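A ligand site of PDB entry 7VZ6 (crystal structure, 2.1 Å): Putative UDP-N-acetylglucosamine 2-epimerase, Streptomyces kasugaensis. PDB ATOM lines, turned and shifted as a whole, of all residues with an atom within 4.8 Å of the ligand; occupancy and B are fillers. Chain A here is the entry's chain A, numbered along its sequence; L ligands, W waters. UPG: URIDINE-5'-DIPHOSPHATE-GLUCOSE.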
ATOM      1  N   ARG A  14       7.185  -0.744  -6.071  1.00  0.00           N
ATOM      2  CA  ARG A  14       6.895  -1.347  -4.748  1.00  0.00           C
ATOM      3  C   ARG A  14       6.160  -2.688  -4.900  1.00  0.00           C
ATOM      4  O   ARG A  14       6.619  -3.688  -4.351  1.00  0.00           O
ATOM      5  CB  ARG A  14       6.110  -0.345  -3.884  1.00  0.00           C
ATOM      6  CG  ARG A  14       5.248  -1.007  -2.815  1.00  0.00           C
ATOM      7  CD  ARG A  14       4.553  -0.078  -1.838  1.00  0.00           C
ATOM      8  NE  ARG A  14       3.366   0.519  -2.405  1.00  0.00           N
ATOM      9  CZ  ARG A  14       2.751   1.614  -1.940  1.00  0.00           C
ATOM     10  NH1 ARG A  14       3.181   2.221  -0.837  1.00  0.00           N
ATOM     11  NH2 ARG A  14       1.667   2.069  -2.546  1.00  0.00           N
ATOM     12  N   PRO A  15       5.007  -2.780  -5.594  1.00  0.00           N
ATOM     13  CA  PRO A  15       4.275  -4.043  -5.646  1.00  0.00           C
ATOM     14  C   PRO A  15       5.127  -5.171  -6.238  1.00  0.00           C
ATOM     15  O   PRO A  15       5.007  -6.290  -5.732  1.00  0.00           O
ATOM     16  CB  PRO A  15       3.023  -3.762  -6.478  1.00  0.00           C
ATOM     17  CG  PRO A  15       3.282  -2.438  -7.159  1.00  0.00           C
ATOM     18  CD  PRO A  15       4.288  -1.699  -6.305  1.00  0.00           C
ATOM     19  N   GLU A  16       5.930  -4.885  -7.261  1.00  0.00           N
ATOM     20  CA  GLU A  16       6.850  -5.869  -7.887  1.00  0.00           C
ATOM     21  C   GLU A  16       7.880  -6.323  -6.855  1.00  0.00           C
ATOM     22  O   GLU A  16       8.102  -7.542  -6.740  1.00  0.00           O
ATOM     23  CB  GLU A  16       7.612  -5.334  -9.094  1.00  0.00           C
ATOM     24  CG  GLU A  16       6.760  -5.023 -10.321  1.00  0.00           C
ATOM     25  CD  GLU A  16       7.577  -4.271 -11.369  1.00  0.00           C
ATOM     26  OE1 GLU A  16       7.957  -3.097 -11.108  1.00  0.00           O
ATOM     27  OE2 GLU A  16       7.882  -4.869 -12.399  1.00  0.00           O
ATOM     28  N   ILE A  18       7.796  -6.265  -3.581  1.00  0.00           N
ATOM     29  CA  ILE A  18       7.125  -7.062  -2.509  1.00  0.00           C
ATOM     30  C   ILE A  18       6.922  -8.491  -3.012  1.00  0.00           C
ATOM     31  O   ILE A  18       7.247  -9.436  -2.274  1.00  0.00           O
ATOM     32  CB  ILE A  18       5.818  -6.405  -2.052  1.00  0.00           C
ATOM     33  CG1 ILE A  18       6.124  -5.124  -1.274  1.00  0.00           C
ATOM     34  CG2 ILE A  18       4.944  -7.380  -1.247  1.00  0.00           C
ATOM     35  CD1 ILE A  18       4.908  -4.239  -1.078  1.00  0.00           C
ATOM     36  N   LYS A  19       6.424  -8.649  -4.244  1.00  0.00           N
ATOM     37  CA  LYS A  19       6.073  -9.995  -4.753  1.00  0.00           C
ATOM     38  C   LYS A  19       7.344 -10.757  -5.173  1.00  0.00           C
ATOM     39  O   LYS A  19       7.334 -11.985  -5.090  1.00  0.00           O
ATOM     40  CB  LYS A  19       5.010  -9.859  -5.843  1.00  0.00           C
ATOM     41  CG  LYS A  19       3.616  -9.707  -5.264  1.00  0.00           C
ATOM     42  CD  LYS A  19       2.529  -9.246  -6.233  1.00  0.00           C
ATOM     43  CE  LYS A  19       1.154  -9.390  -5.608  1.00  0.00           C
ATOM     44  NZ  LYS A  19       0.054  -8.873  -6.446  1.00  0.00           N
ATOM     45  N   GLN A  97       7.799  -9.809 -13.125  1.00  0.00           N
ATOM     46  CA  GLN A  97       6.612  -9.970 -12.266  1.00  0.00           C
ATOM     47  C   GLN A  97       5.515  -9.028 -12.729  1.00  0.00           C
ATOM     48  O   GLN A  97       5.809  -7.901 -13.088  1.00  0.00           O
ATOM     49  CB  GLN A  97       6.980  -9.696 -10.809  1.00  0.00           C
ATOM     50  CG  GLN A  97       5.909 -10.087  -9.818  1.00  0.00           C
ATOM     51  CD  GLN A  97       4.785  -9.080  -9.739  1.00  0.00           C
ATOM     52  OE1 GLN A  97       4.980  -7.884  -9.905  1.00  0.00           O
ATOM     53  NE2 GLN A  97       3.601  -9.570  -9.477  1.00  0.00           N
ATOM     54  N   GLY A  98       4.276  -9.517 -12.722  1.00  0.00           N
ATOM     55  CA  GLY A  98       3.094  -8.651 -12.780  1.00  0.00           C
ATOM     56  C   GLY A  98       2.853  -8.080 -14.160  1.00  0.00           C
ATOM     57  O   GLY A  98       3.007  -8.817 -15.156  1.00  0.00           O
ATOM     58  N   ASP A  99       2.468  -6.810 -14.215  1.00  0.00           N
ATOM     59  CA  ASP A  99       1.830  -6.243 -15.422  1.00  0.00           C
ATOM     60  C   ASP A  99       2.533  -4.956 -15.854  1.00  0.00           C
ATOM     61  O   ASP A  99       1.957  -4.263 -16.675  1.00  0.00           O
ATOM     62  CB  ASP A  99       0.343  -5.998 -15.149  1.00  0.00           C
ATOM     63  CG  ASP A  99       0.079  -4.978 -14.048  1.00  0.00           C
ATOM     64  OD1 ASP A  99       1.057  -4.348 -13.547  1.00  0.00           O
ATOM     65  OD2 ASP A  99      -1.117  -4.785 -13.708  1.00  0.00           O
ATOM     66  N   THR A 100       3.692  -4.629 -15.308  1.00  0.00           N
ATOM     67  CA  THR A 100       4.349  -3.320 -15.543  1.00  0.00           C
ATOM     68  C   THR A 100       4.933  -3.261 -16.950  1.00  0.00           C
ATOM     69  O   THR A 100       5.237  -4.299 -17.560  1.00  0.00           O
ATOM     70  CB  THR A 100       5.439  -3.013 -14.512  1.00  0.00           C
ATOM     71  OG1 THR A 100       6.402  -4.060 -14.586  1.00  0.00           O
ATOM     72  CG2 THR A 100       4.870  -2.880 -13.114  1.00  0.00           C
ATOM     73  N   GLU A 121       3.516 -14.437 -11.287  1.00  0.00           N
ATOM     74  CA  GLU A 121       2.115 -13.980 -11.210  1.00  0.00           C
ATOM     75  C   GLU A 121       1.557 -13.842 -12.644  1.00  0.00           C
ATOM     76  O   GLU A 121       1.193 -12.724 -13.055  1.00  0.00           O
ATOM     77  CB  GLU A 121       2.010 -12.695 -10.409  1.00  0.00           C
ATOM     78  CG  GLU A 121       0.577 -12.348 -10.067  1.00  0.00           C
ATOM     79  CD  GLU A 121       0.381 -10.905  -9.627  1.00  0.00           C
ATOM     80  OE1 GLU A 121       0.430 -10.687  -8.425  1.00  0.00           O
ATOM     81  OE2 GLU A 121       0.188 -10.000 -10.518  1.00  0.00           O
ATOM     82  N   LEU A 124      -3.363 -13.408 -14.912  1.00  0.00           N
ATOM     83  CA  LEU A 124      -4.491 -12.586 -14.391  1.00  0.00           C
ATOM     84  C   LEU A 124      -5.097 -11.821 -15.566  1.00  0.00           C
ATOM     85  O   LEU A 124      -4.344 -11.233 -16.373  1.00  0.00           O
ATOM     86  CB  LEU A 124      -4.029 -11.652 -13.281  1.00  0.00           C
ATOM     87  CG  LEU A 124      -3.409 -12.314 -12.058  1.00  0.00           C
ATOM     88  CD1 LEU A 124      -3.274 -11.299 -10.931  1.00  0.00           C
ATOM     89  CD2 LEU A 124      -4.245 -13.450 -11.574  1.00  0.00           C
ATOM     90  N   ARG A 139       0.521  -7.802 -19.923  1.00  0.00           N
ATOM     91  CA  ARG A 139       0.350  -9.216 -19.490  1.00  0.00           C
ATOM     92  C   ARG A 139       0.302 -10.142 -20.718  1.00  0.00           C
ATOM     93  O   ARG A 139       0.966 -11.188 -20.684  1.00  0.00           O
ATOM     94  CB  ARG A 139      -0.904  -9.407 -18.657  1.00  0.00           C
ATOM     95  CG  ARG A 139      -0.750  -8.904 -17.239  1.00  0.00           C
ATOM     96  CD  ARG A 139      -1.913  -9.317 -16.373  1.00  0.00           C
ATOM     97  NE  ARG A 139      -1.555  -9.127 -14.986  1.00  0.00           N
ATOM     98  CZ  ARG A 139      -0.817  -9.981 -14.259  1.00  0.00           C
ATOM     99  NH1 ARG A 139      -0.392 -11.113 -14.777  1.00  0.00           N
ATOM    100  NH2 ARG A 139      -0.528  -9.675 -13.010  1.00  0.00           N
ATOM    101  N   VAL A 177       2.941 -13.015  -2.781  1.00  0.00           N
ATOM    102  CA  VAL A 177       2.518 -11.953  -1.832  1.00  0.00           C
ATOM    103  C   VAL A 177       2.144 -12.607  -0.490  1.00  0.00           C
ATOM    104  O   VAL A 177       2.359 -11.973   0.555  1.00  0.00           O
ATOM    105  CB  VAL A 177       1.387 -11.054  -2.354  1.00  0.00           C
ATOM    106  CG1 VAL A 177       0.028 -11.691  -2.341  1.00  0.00           C
ATOM    107  CG2 VAL A 177       1.361  -9.742  -1.606  1.00  0.00           C
ATOM    108  N   THR A 209      -7.023   2.121   0.588  1.00  0.00           N
ATOM    109  CA  THR A 209      -5.993   2.527  -0.390  1.00  0.00           C
ATOM    110  C   THR A 209      -6.654   2.653  -1.759  1.00  0.00           C
ATOM    111  O   THR A 209      -7.471   1.799  -2.135  1.00  0.00           O
ATOM    112  CB  THR A 209      -4.775   1.590  -0.461  1.00  0.00           C
ATOM    113  OG1 THR A 209      -5.115   0.359  -1.079  1.00  0.00           O
ATOM    114  CG2 THR A 209      -4.172   1.346   0.904  1.00  0.00           C
ATOM    115  N   HIS A 211      -5.328   4.160  -5.811  1.00  0.00           N
ATOM    116  CA  HIS A 211      -4.216   4.720  -6.611  1.00  0.00           C
ATOM    117  C   HIS A 211      -4.457   4.705  -8.127  1.00  0.00           C
ATOM    118  O   HIS A 211      -3.665   5.340  -8.796  1.00  0.00           O
ATOM    119  CB  HIS A 211      -2.893   3.989  -6.296  1.00  0.00           C
ATOM    120  CG  HIS A 211      -2.810   2.610  -6.833  1.00  0.00           C
ATOM    121  ND1 HIS A 211      -2.447   2.321  -8.131  1.00  0.00           N
ATOM    122  CD2 HIS A 211      -2.990   1.432  -6.222  1.00  0.00           C
ATOM    123  CE1 HIS A 211      -2.420   1.000  -8.297  1.00  0.00           C
ATOM    124  NE2 HIS A 211      -2.782   0.430  -7.132  1.00  0.00           N
ATOM    125  N   ARG A 212      -5.461   4.018  -8.658  1.00  0.00           N
ATOM    126  CA  ARG A 212      -5.464   3.735 -10.118  1.00  0.00           C
ATOM    127  C   ARG A 212      -5.748   5.017 -10.919  1.00  0.00           C
ATOM    128  O   ARG A 212      -6.654   5.752 -10.578  1.00  0.00           O
ATOM    129  CB  ARG A 212      -6.437   2.613 -10.471  1.00  0.00           C
ATOM    130  CG  ARG A 212      -5.900   1.250 -10.090  1.00  0.00           C
ATOM    131  CD  ARG A 212      -6.768   0.114 -10.507  1.00  0.00           C
ATOM    132  NE  ARG A 212      -6.255  -1.023  -9.761  1.00  0.00           N
ATOM    133  CZ  ARG A 212      -5.237  -1.795 -10.115  1.00  0.00           C
ATOM    134  NH1 ARG A 212      -4.576  -1.582 -11.244  1.00  0.00           N
ATOM    135  NH2 ARG A 212      -4.896  -2.791  -9.316  1.00  0.00           N
ATOM    136  N   PRO A 242      -3.435   5.467   3.887  1.00  0.00           N
ATOM    137  CA  PRO A 242      -2.085   5.661   3.386  1.00  0.00           C
ATOM    138  C   PRO A 242      -2.211   6.090   1.917  1.00  0.00           C
ATOM    139  O   PRO A 242      -2.949   5.475   1.187  1.00  0.00           O
ATOM    140  CB  PRO A 242      -1.405   4.280   3.533  1.00  0.00           C
ATOM    141  CG  PRO A 242      -2.323   3.535   4.461  1.00  0.00           C
ATOM    142  CD  PRO A 242      -3.712   4.043   4.115  1.00  0.00           C
ATOM    143  N   HIS A 244      -1.090   6.913  -1.913  1.00  0.00           N
ATOM    144  CA  HIS A 244      -0.171   6.649  -3.054  1.00  0.00           C
ATOM    145  C   HIS A 244       0.685   7.900  -3.300  1.00  0.00           C
ATOM    146  O   HIS A 244       0.193   9.014  -3.199  1.00  0.00           O
ATOM    147  CB  HIS A 244      -0.991   6.211  -4.268  1.00  0.00           C
ATOM    148  CG  HIS A 244      -0.161   5.717  -5.410  1.00  0.00           C
ATOM    149  ND1 HIS A 244       0.379   4.435  -5.433  1.00  0.00           N
ATOM    150  CD2 HIS A 244       0.223   6.323  -6.549  1.00  0.00           C
ATOM    151  CE1 HIS A 244       1.073   4.294  -6.554  1.00  0.00           C
ATOM    152  NE2 HIS A 244       0.994   5.430  -7.245  1.00  0.00           N
ATOM    153  N   PRO A 268       2.872   6.859   2.642  1.00  0.00           N
ATOM    154  CA  PRO A 268       3.029   5.432   2.364  1.00  0.00           C
ATOM    155  C   PRO A 268       3.678   4.749   3.566  1.00  0.00           C
ATOM    156  O   PRO A 268       4.603   5.274   4.105  1.00  0.00           O
ATOM    157  CB  PRO A 268       3.955   5.383   1.148  1.00  0.00           C
ATOM    158  CG  PRO A 268       3.774   6.740   0.460  1.00  0.00           C
ATOM    159  CD  PRO A 268       3.373   7.717   1.559  1.00  0.00           C
ATOM    160  N   LEU A 269       3.148   3.599   3.972  1.00  0.00           N
ATOM    161  CA  LEU A 269       3.661   2.846   5.132  1.00  0.00           C
ATOM    162  C   LEU A 269       4.644   1.786   4.640  1.00  0.00           C
ATOM    163  O   LEU A 269       4.399   1.171   3.600  1.00  0.00           O
ATOM    164  CB  LEU A 269       2.482   2.229   5.880  1.00  0.00           C
ATOM    165  CG  LEU A 269       1.451   3.203   6.401  1.00  0.00           C
ATOM    166  CD1 LEU A 269       0.299   2.479   7.066  1.00  0.00           C
ATOM    167  CD2 LEU A 269       2.090   4.154   7.374  1.00  0.00           C
ATOM    168  N   ARG A 270       5.702   1.539   5.398  1.00  0.00           N
ATOM    169  CA  ARG A 270       6.561   0.352   5.265  1.00  0.00           C
ATOM    170  C   ARG A 270       5.650  -0.882   5.305  1.00  0.00           C
ATOM    171  O   ARG A 270       4.647  -0.884   6.056  1.00  0.00           O
ATOM    172  CB  ARG A 270       7.652   0.388   6.341  1.00  0.00           C
ATOM    173  CG  ARG A 270       8.675  -0.726   6.215  1.00  0.00           C
ATOM    174  CD  ARG A 270       9.912  -0.520   7.041  1.00  0.00           C
ATOM    175  NE  ARG A 270       9.551  -0.401   8.452  1.00  0.00           N
ATOM    176  CZ  ARG A 270      10.384  -0.562   9.461  1.00  0.00           C
ATOM    177  NH1 ARG A 270      11.660  -0.855   9.257  1.00  0.00           N
ATOM    178  NH2 ARG A 270       9.933  -0.413  10.700  1.00  0.00           N
ATOM    179  N   TYR A 271       5.998  -1.893   4.507  1.00  0.00           N
ATOM    180  CA  TYR A 271       5.127  -3.073   4.251  1.00  0.00           C
ATOM    181  C   TYR A 271       4.749  -3.761   5.581  1.00  0.00           C
ATOM    182  O   TYR A 271       3.599  -4.136   5.770  1.00  0.00           O
ATOM    183  CB  TYR A 271       5.815  -3.988   3.244  1.00  0.00           C
ATOM    184  CG  TYR A 271       4.973  -5.184   2.875  1.00  0.00           C
ATOM    185  CD1 TYR A 271       3.752  -5.022   2.267  1.00  0.00           C
ATOM    186  CD2 TYR A 271       5.430  -6.473   3.109  1.00  0.00           C
ATOM    187  CE1 TYR A 271       2.980  -6.107   1.916  1.00  0.00           C
ATOM    188  CE2 TYR A 271       4.653  -7.576   2.781  1.00  0.00           C
ATOM    189  CZ  TYR A 271       3.425  -7.386   2.177  1.00  0.00           C
ATOM    190  OH  TYR A 271       2.653  -8.457   1.832  1.00  0.00           O
ATOM    191  N   PHE A 274       2.181  -1.697   7.334  1.00  0.00           N
ATOM    192  CA  PHE A 274       0.937  -1.716   6.542  1.00  0.00           C
ATOM    193  C   PHE A 274       0.170  -3.023   6.813  1.00  0.00           C
ATOM    194  O   PHE A 274      -1.055  -2.991   7.010  1.00  0.00           O
ATOM    195  CB  PHE A 274       1.236  -1.517   5.047  1.00  0.00           C
ATOM    196  CG  PHE A 274      -0.017  -1.473   4.221  1.00  0.00           C
ATOM    197  CD1 PHE A 274      -0.856  -0.368   4.248  1.00  0.00           C
ATOM    198  CD2 PHE A 274      -0.355  -2.531   3.419  1.00  0.00           C
ATOM    199  CE1 PHE A 274      -2.009  -0.335   3.486  1.00  0.00           C
ATOM    200  CE2 PHE A 274      -1.519  -2.514   2.673  1.00  0.00           C
ATOM    201  CZ  PHE A 274      -2.341  -1.408   2.699  1.00  0.00           C
ATOM    202  N   ILE A 275       0.883  -4.150   6.839  1.00  0.00           N
ATOM    203  CA  ILE A 275       0.274  -5.486   7.119  1.00  0.00           C
ATOM    204  C   ILE A 275      -0.265  -5.512   8.558  1.00  0.00           C
ATOM    205  O   ILE A 275      -1.403  -6.014   8.750  1.00  0.00           O
ATOM    206  CB  ILE A 275       1.250  -6.623   6.790  1.00  0.00           C
ATOM    207  CG1 ILE A 275       1.560  -6.684   5.267  1.00  0.00           C
ATOM    208  CG2 ILE A 275       0.688  -7.933   7.301  1.00  0.00           C
ATOM    209  CD1 ILE A 275       0.355  -6.950   4.389  1.00  0.00           C
ATOM    210  N   MET A 278      -3.493  -3.569   8.587  1.00  0.00           N
ATOM    211  CA  MET A 278      -4.549  -4.311   7.869  1.00  0.00           C
ATOM    212  C   MET A 278      -5.135  -5.378   8.807  1.00  0.00           C
ATOM    213  O   MET A 278      -6.369  -5.574   8.775  1.00  0.00           O
ATOM    214  CB  MET A 278      -3.989  -4.987   6.609  1.00  0.00           C
ATOM    215  CG  MET A 278      -5.061  -5.559   5.678  1.00  0.00           C
ATOM    216  SD  MET A 278      -4.258  -6.429   4.270  1.00  0.00           S
ATOM    217  CE  MET A 278      -3.304  -5.143   3.509  1.00  0.00           C
ATOM    218  N   ASP A 287      -8.454  -0.330  -4.355  1.00  0.00           N
ATOM    219  CA  ASP A 287      -8.354  -0.699  -5.772  1.00  0.00           C
ATOM    220  C   ASP A 287      -7.020  -1.403  -6.027  1.00  0.00           C
ATOM    221  O   ASP A 287      -6.704  -1.653  -7.214  1.00  0.00           O
ATOM    222  CB  ASP A 287      -8.577   0.498  -6.688  1.00  0.00           C
ATOM    223  CG  ASP A 287      -7.538   1.581  -6.694  1.00  0.00           C
ATOM    224  OD1 ASP A 287      -6.537   1.464  -5.981  1.00  0.00           O
ATOM    225  OD2 ASP A 287      -7.749   2.547  -7.433  1.00  0.00           O
ATOM    226  N   SER A 288      -6.289  -1.746  -4.974  1.00  0.00           N
ATOM    227  CA  SER A 288      -4.989  -2.452  -5.080  1.00  0.00           C
ATOM    228  C   SER A 288      -5.205  -3.941  -5.407  1.00  0.00           C
ATOM    229  O   SER A 288      -6.061  -4.573  -4.766  1.00  0.00           O
ATOM    230  CB  SER A 288      -4.196  -2.302  -3.806  1.00  0.00           C
ATOM    231  OG  SER A 288      -3.131  -3.259  -3.747  1.00  0.00           O
ATOM    232  N   GLY A 289      -4.452  -4.475  -6.353  1.00  0.00           N
ATOM    233  CA  GLY A 289      -4.410  -5.925  -6.643  1.00  0.00           C
ATOM    234  C   GLY A 289      -3.872  -6.715  -5.452  1.00  0.00           C
ATOM    235  O   GLY A 289      -4.520  -7.684  -5.075  1.00  0.00           O
ATOM    236  N   GLY A 290      -2.727  -6.332  -4.910  1.00  0.00           N
ATOM    237  CA  GLY A 290      -2.090  -7.026  -3.784  1.00  0.00           C
ATOM    238  C   GLY A 290      -2.950  -7.029  -2.536  1.00  0.00           C
ATOM    239  O   GLY A 290      -3.014  -8.062  -1.860  1.00  0.00           O
ATOM    240  N   VAL A 291      -3.619  -5.914  -2.235  1.00  0.00           N
ATOM    241  CA  VAL A 291      -4.460  -5.823  -1.003  1.00  0.00           C
ATOM    242  C   VAL A 291      -5.664  -6.754  -1.165  1.00  0.00           C
ATOM    243  O   VAL A 291      -6.066  -7.374  -0.180  1.00  0.00           O
ATOM    244  CB  VAL A 291      -4.832  -4.359  -0.669  1.00  0.00           C
ATOM    245  CG1 VAL A 291      -5.748  -4.269   0.543  1.00  0.00           C
ATOM    246  CG2 VAL A 291      -3.584  -3.501  -0.480  1.00  0.00           C
ATOM    247  N   GLU A 294      -4.053  -9.909   0.034  1.00  0.00           N
ATOM    248  CA  GLU A 294      -3.560  -9.875   1.447  1.00  0.00           C
ATOM    249  C   GLU A 294      -4.764  -9.872   2.406  1.00  0.00           C
ATOM    250  O   GLU A 294      -4.743 -10.661   3.352  1.00  0.00           O
ATOM    251  CB  GLU A 294      -2.662  -8.668   1.680  1.00  0.00           C
ATOM    252  CG  GLU A 294      -1.367  -8.738   0.890  1.00  0.00           C
ATOM    253  CD  GLU A 294      -0.640  -7.427   0.640  1.00  0.00           C
ATOM    254  OE1 GLU A 294      -1.291  -6.377   0.747  1.00  0.00           O
ATOM    255  OE2 GLU A 294       0.584  -7.481   0.338  1.00  0.00           O
ATOM    256  N   GLU A 310      -8.976  -8.394 -11.485  1.00  0.00           N
ATOM    257  CA  GLU A 310      -8.145  -9.541 -11.905  1.00  0.00           C
ATOM    258  C   GLU A 310      -8.134 -10.609 -10.815  1.00  0.00           C
ATOM    259  O   GLU A 310      -7.440 -11.613 -11.019  1.00  0.00           O
ATOM    260  CB  GLU A 310      -6.706  -9.059 -12.147  1.00  0.00           C
ATOM    261  CG  GLU A 310      -6.546  -8.273 -13.421  1.00  0.00           C
ATOM    262  CD  GLU A 310      -5.129  -7.800 -13.662  1.00  0.00           C
ATOM    263  OE1 GLU A 310      -4.462  -7.367 -12.667  1.00  0.00           O
ATOM    264  OE2 GLU A 310      -4.683  -7.859 -14.845  1.00  0.00           O
ATOM    265  N   ARG A 311      -8.854 -10.392  -9.707  1.00  0.00           N
ATOM    266  CA  ARG A 311      -8.973 -11.400  -8.607  1.00  0.00           C
ATOM    267  C   ARG A 311     -10.419 -11.877  -8.493  1.00  0.00           C
ATOM    268  O   ARG A 311     -11.079 -11.613  -7.496  1.00  0.00           O
ATOM    269  CB  ARG A 311      -8.447 -10.812  -7.304  1.00  0.00           C
ATOM    270  CG  ARG A 311      -6.932 -10.803  -7.202  1.00  0.00           C
ATOM    271  CD  ARG A 311      -6.275  -9.606  -7.896  1.00  0.00           C
ATOM    272  NE  ARG A 311      -4.830  -9.720  -7.818  1.00  0.00           N
ATOM    273  CZ  ARG A 311      -3.957  -8.943  -8.450  1.00  0.00           C
ATOM    274  NH1 ARG A 311      -4.337  -7.969  -9.253  1.00  0.00           N
ATOM    275  NH2 ARG A 311      -2.674  -9.175  -8.318  1.00  0.00           N
HETATM  276  N1  UPG L   1       1.393  -1.410   0.517  1.00  0.00           N
HETATM  277  C2  UPG L   1       2.389  -0.986   1.375  1.00  0.00           C
HETATM  278  N3  UPG L   1       2.198   0.238   1.948  1.00  0.00           N
HETATM  279  C4  UPG L   1       1.146   1.112   1.718  1.00  0.00           C
HETATM  280  C5  UPG L   1       0.187   0.622   0.786  1.00  0.00           C
HETATM  281  C6  UPG L   1       0.337  -0.575   0.219  1.00  0.00           C
HETATM  282  O2  UPG L   1       3.374  -1.648   1.630  1.00  0.00           O
HETATM  283  O4  UPG L   1       1.111   2.190   2.316  1.00  0.00           O
HETATM  284  C1C UPG L   1       1.580  -2.691  -0.186  1.00  0.00           C
HETATM  285  C2C UPG L   1       0.377  -3.624  -0.213  1.00  0.00           C
HETATM  286  O2C UPG L   1       0.353  -4.374   0.979  1.00  0.00           O
HETATM  287  C3C UPG L   1       0.725  -4.472  -1.456  1.00  0.00           C
HETATM  288  C4C UPG L   1       1.298  -3.397  -2.395  1.00  0.00           C
HETATM  289  O4C UPG L   1       1.818  -2.367  -1.535  1.00  0.00           O
HETATM  290  O3C UPG L   1       1.657  -5.546  -1.259  1.00  0.00           O
HETATM  291  C5C UPG L   1       0.285  -2.779  -3.342  1.00  0.00           C
HETATM  292  O5C UPG L   1       0.941  -1.850  -4.247  1.00  0.00           O
HETATM  293  PA  UPG L   1      -0.012  -1.021  -5.205  1.00  0.00           P
HETATM  294  O1A UPG L   1       0.682   0.217  -5.569  1.00  0.00           O
HETATM  295  O2A UPG L   1      -1.347  -0.880  -4.583  1.00  0.00           O
HETATM  296  O3A UPG L   1      -0.113  -1.956  -6.516  1.00  0.00           O
HETATM  297  PB  UPG L   1      -1.141  -3.127  -6.886  1.00  0.00           P
HETATM  298  O1B UPG L   1      -2.381  -2.491  -7.407  1.00  0.00           O
HETATM  299  O2B UPG L   1      -1.268  -4.039  -5.709  1.00  0.00           O
HETATM  300  O3B UPG L   1      -0.323  -3.989  -7.962  1.00  0.00           O
HETATM  301  C1' UPG L   1      -0.400  -3.873  -9.376  1.00  0.00           C
HETATM  302  C2' UPG L   1      -1.319  -4.951  -9.904  1.00  0.00           C
HETATM  303  C3' UPG L   1      -0.759  -6.303  -9.510  1.00  0.00           C
HETATM  304  C4' UPG L   1       0.631  -6.509 -10.055  1.00  0.00           C
HETATM  305  C5' UPG L   1       1.527  -5.333  -9.656  1.00  0.00           C
HETATM  306  C6' UPG L   1       2.846  -5.297 -10.406  1.00  0.00           C
HETATM  307  O2' UPG L   1      -2.645  -4.756  -9.429  1.00  0.00           O
HETATM  308  O3' UPG L   1      -1.599  -7.323 -10.021  1.00  0.00           O
HETATM  309  O4' UPG L   1       1.123  -7.724  -9.545  1.00  0.00           O
HETATM  310  O5' UPG L   1       0.862  -4.072  -9.964  1.00  0.00           O
HETATM  311  O6' UPG L   1       2.596  -5.319 -11.808  1.00  0.00           O
HETATM  312  O   HOH W   1       1.198   0.848  -8.294  1.00  0.00           O
HETATM  313  O   HOH W   2       1.184  -2.072 -12.391  1.00  0.00           O
HETATM  314  O   HOH W   3       0.651   4.097  -0.127  1.00  0.00           O
HETATM  315  O   HOH W   4       2.400  -6.392  -3.917  1.00  0.00           O
HETATM  316  O   HOH W   5       0.483  -6.220  -5.849  1.00  0.00           O
HETATM  317  O   HOH W   6      -2.178   0.106  -2.064  1.00  0.00           O
HETATM  318  O   HOH W   7      -4.559  -5.411 -11.099  1.00  0.00           O
HETATM  319  O   HOH W   8      -2.106  -2.848 -12.389  1.00  0.00           O
HETATM  320  O   HOH W   9       6.130  -0.808   1.151  1.00  0.00           O
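The backbone NH (N) of Leu 269 is in hydrogen-bond range of an oxygen (O4) of the ligand, 3.0 Å away. An oxygen (O2B) of the ligand lies within hydrogen-bond range of the side-chain hydroxyl (OG) of Ser 288, at 2.8 Å. O4' of the ligand is in hydrogen-bond range of NE2 of Gln 97 (3.1 Å). NH2 of Arg 212 lies within salt-bridge range of O1B of the ligand (3.2 Å). N of Gly 290 is in hydrogen-bond range of O2B of the ligand (2.8 Å). NE2 of His 211 sits at hydrogen-bond distance from O1B of the ligand, at 3.0 Å. NZ of Lys 19 sits at hydrogen-bond distance from O4' of the ligand (3.5 Å). The side-chain carboxylate (OE2) of Glu 121 sits at hydrogen-bond distance from an oxygen (O4') of the ligand (2.6 Å). The side-chain carboxylate (OD1) of Asp 99 sits at hydrogen-bond distance from an oxygen (O6') of the ligand, at 2.5 Å. O of Leu 269 is in hydrogen-bond range of N3 of the ligand. O6' of the ligand lies within hydrogen-bond range of N of Asp 99, at 2.8 Å. The guanidinium group (NH2) of Arg 14 is in salt-bridge range of an oxygen (O1A) of the ligand. N of Gly 289 lies within hydrogen-bond range of O1B of the ligand, at 3.1 Å. An oxygen (O2C) of the ligand sits at hydrogen-bond distance from the side-chain carboxylate (OE1) of Glu 294, 2.6 Å away. O3' of the ligand sits at hydrogen-bond distance from NH2 of Arg 311 (2.7 Å).
Merely in contact with the ligand: Phe 274, Tyr 271, Pro 15, Pro 242, Gly 98, Ile 18, Thr 100, Pro 268, Glu 310, Glu 16, Arg 139 and Val 291. The nearest printed residue that does not touch the ligand is His 244 (4.2 Å).
Water W7 lies within hydrogen-bond range of OE1 of Glu 310 (2.5 Å), O2' of the ligand (2.6 Å), NH1 of Arg 311 (3.2 Å) and NH2 of Arg 212 (3.2 Å). Water W5 lies within hydrogen-bond range of NZ of Lys 19 (2.8 Å), O2B of the ligand (2.8 Å) and N of Gly 290 (3.3 Å). Water W6 lies within hydrogen-bond range of an oxygen (O2A) of the ligand (2.8 Å) and the side-chain hydroxyl (OG1) of Thr 209 (3.1 Å). Water W4 lies within hydrogen-bond range of an oxygen (O3C) of the ligand (2.9 Å) and the backbone carbonyl oxygen of Pro 15 (3.2 Å). Water W3 bridges O4 of the ligand (3.1 Å) and NH1 of Arg 14 (3.2 Å). Water W2 lies within hydrogen-bond range of the side-chain carboxylate (OD1) of Asp 99 and an oxygen (O5') of the ligand.
The side-chain hydroxyl (OG) of Ser 288 sits at hydrogen-bond distance from the backbone NH (N) of Gly 290. The guanidinium group (NE) of Arg 139 lies within salt-bridge range of the side-chain carboxylate (OE2) of Glu 310, at 3.4 Å. OH of Tyr 271 is in hydrogen-bond range of OE2 of Glu 294 (2.7 Å). OD1 of Asp 287 sits at hydrogen-bond distance from N of His 211 (3.0 Å). OE1 of Glu 121 is in salt-bridge range of NH2 of Arg 311, at 3.5 Å. The side-chain hydroxyl of Thr 100 is in hydrogen-bond range of the side-chain carboxylate of Glu 16 (2.8 Å). The side-chain carboxylate of Glu 310 lies within salt-bridge range of the guanidinium group of Arg 311 (3.5 Å). OG of Ser 288 is in hydrogen-bond range of N of Val 291.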
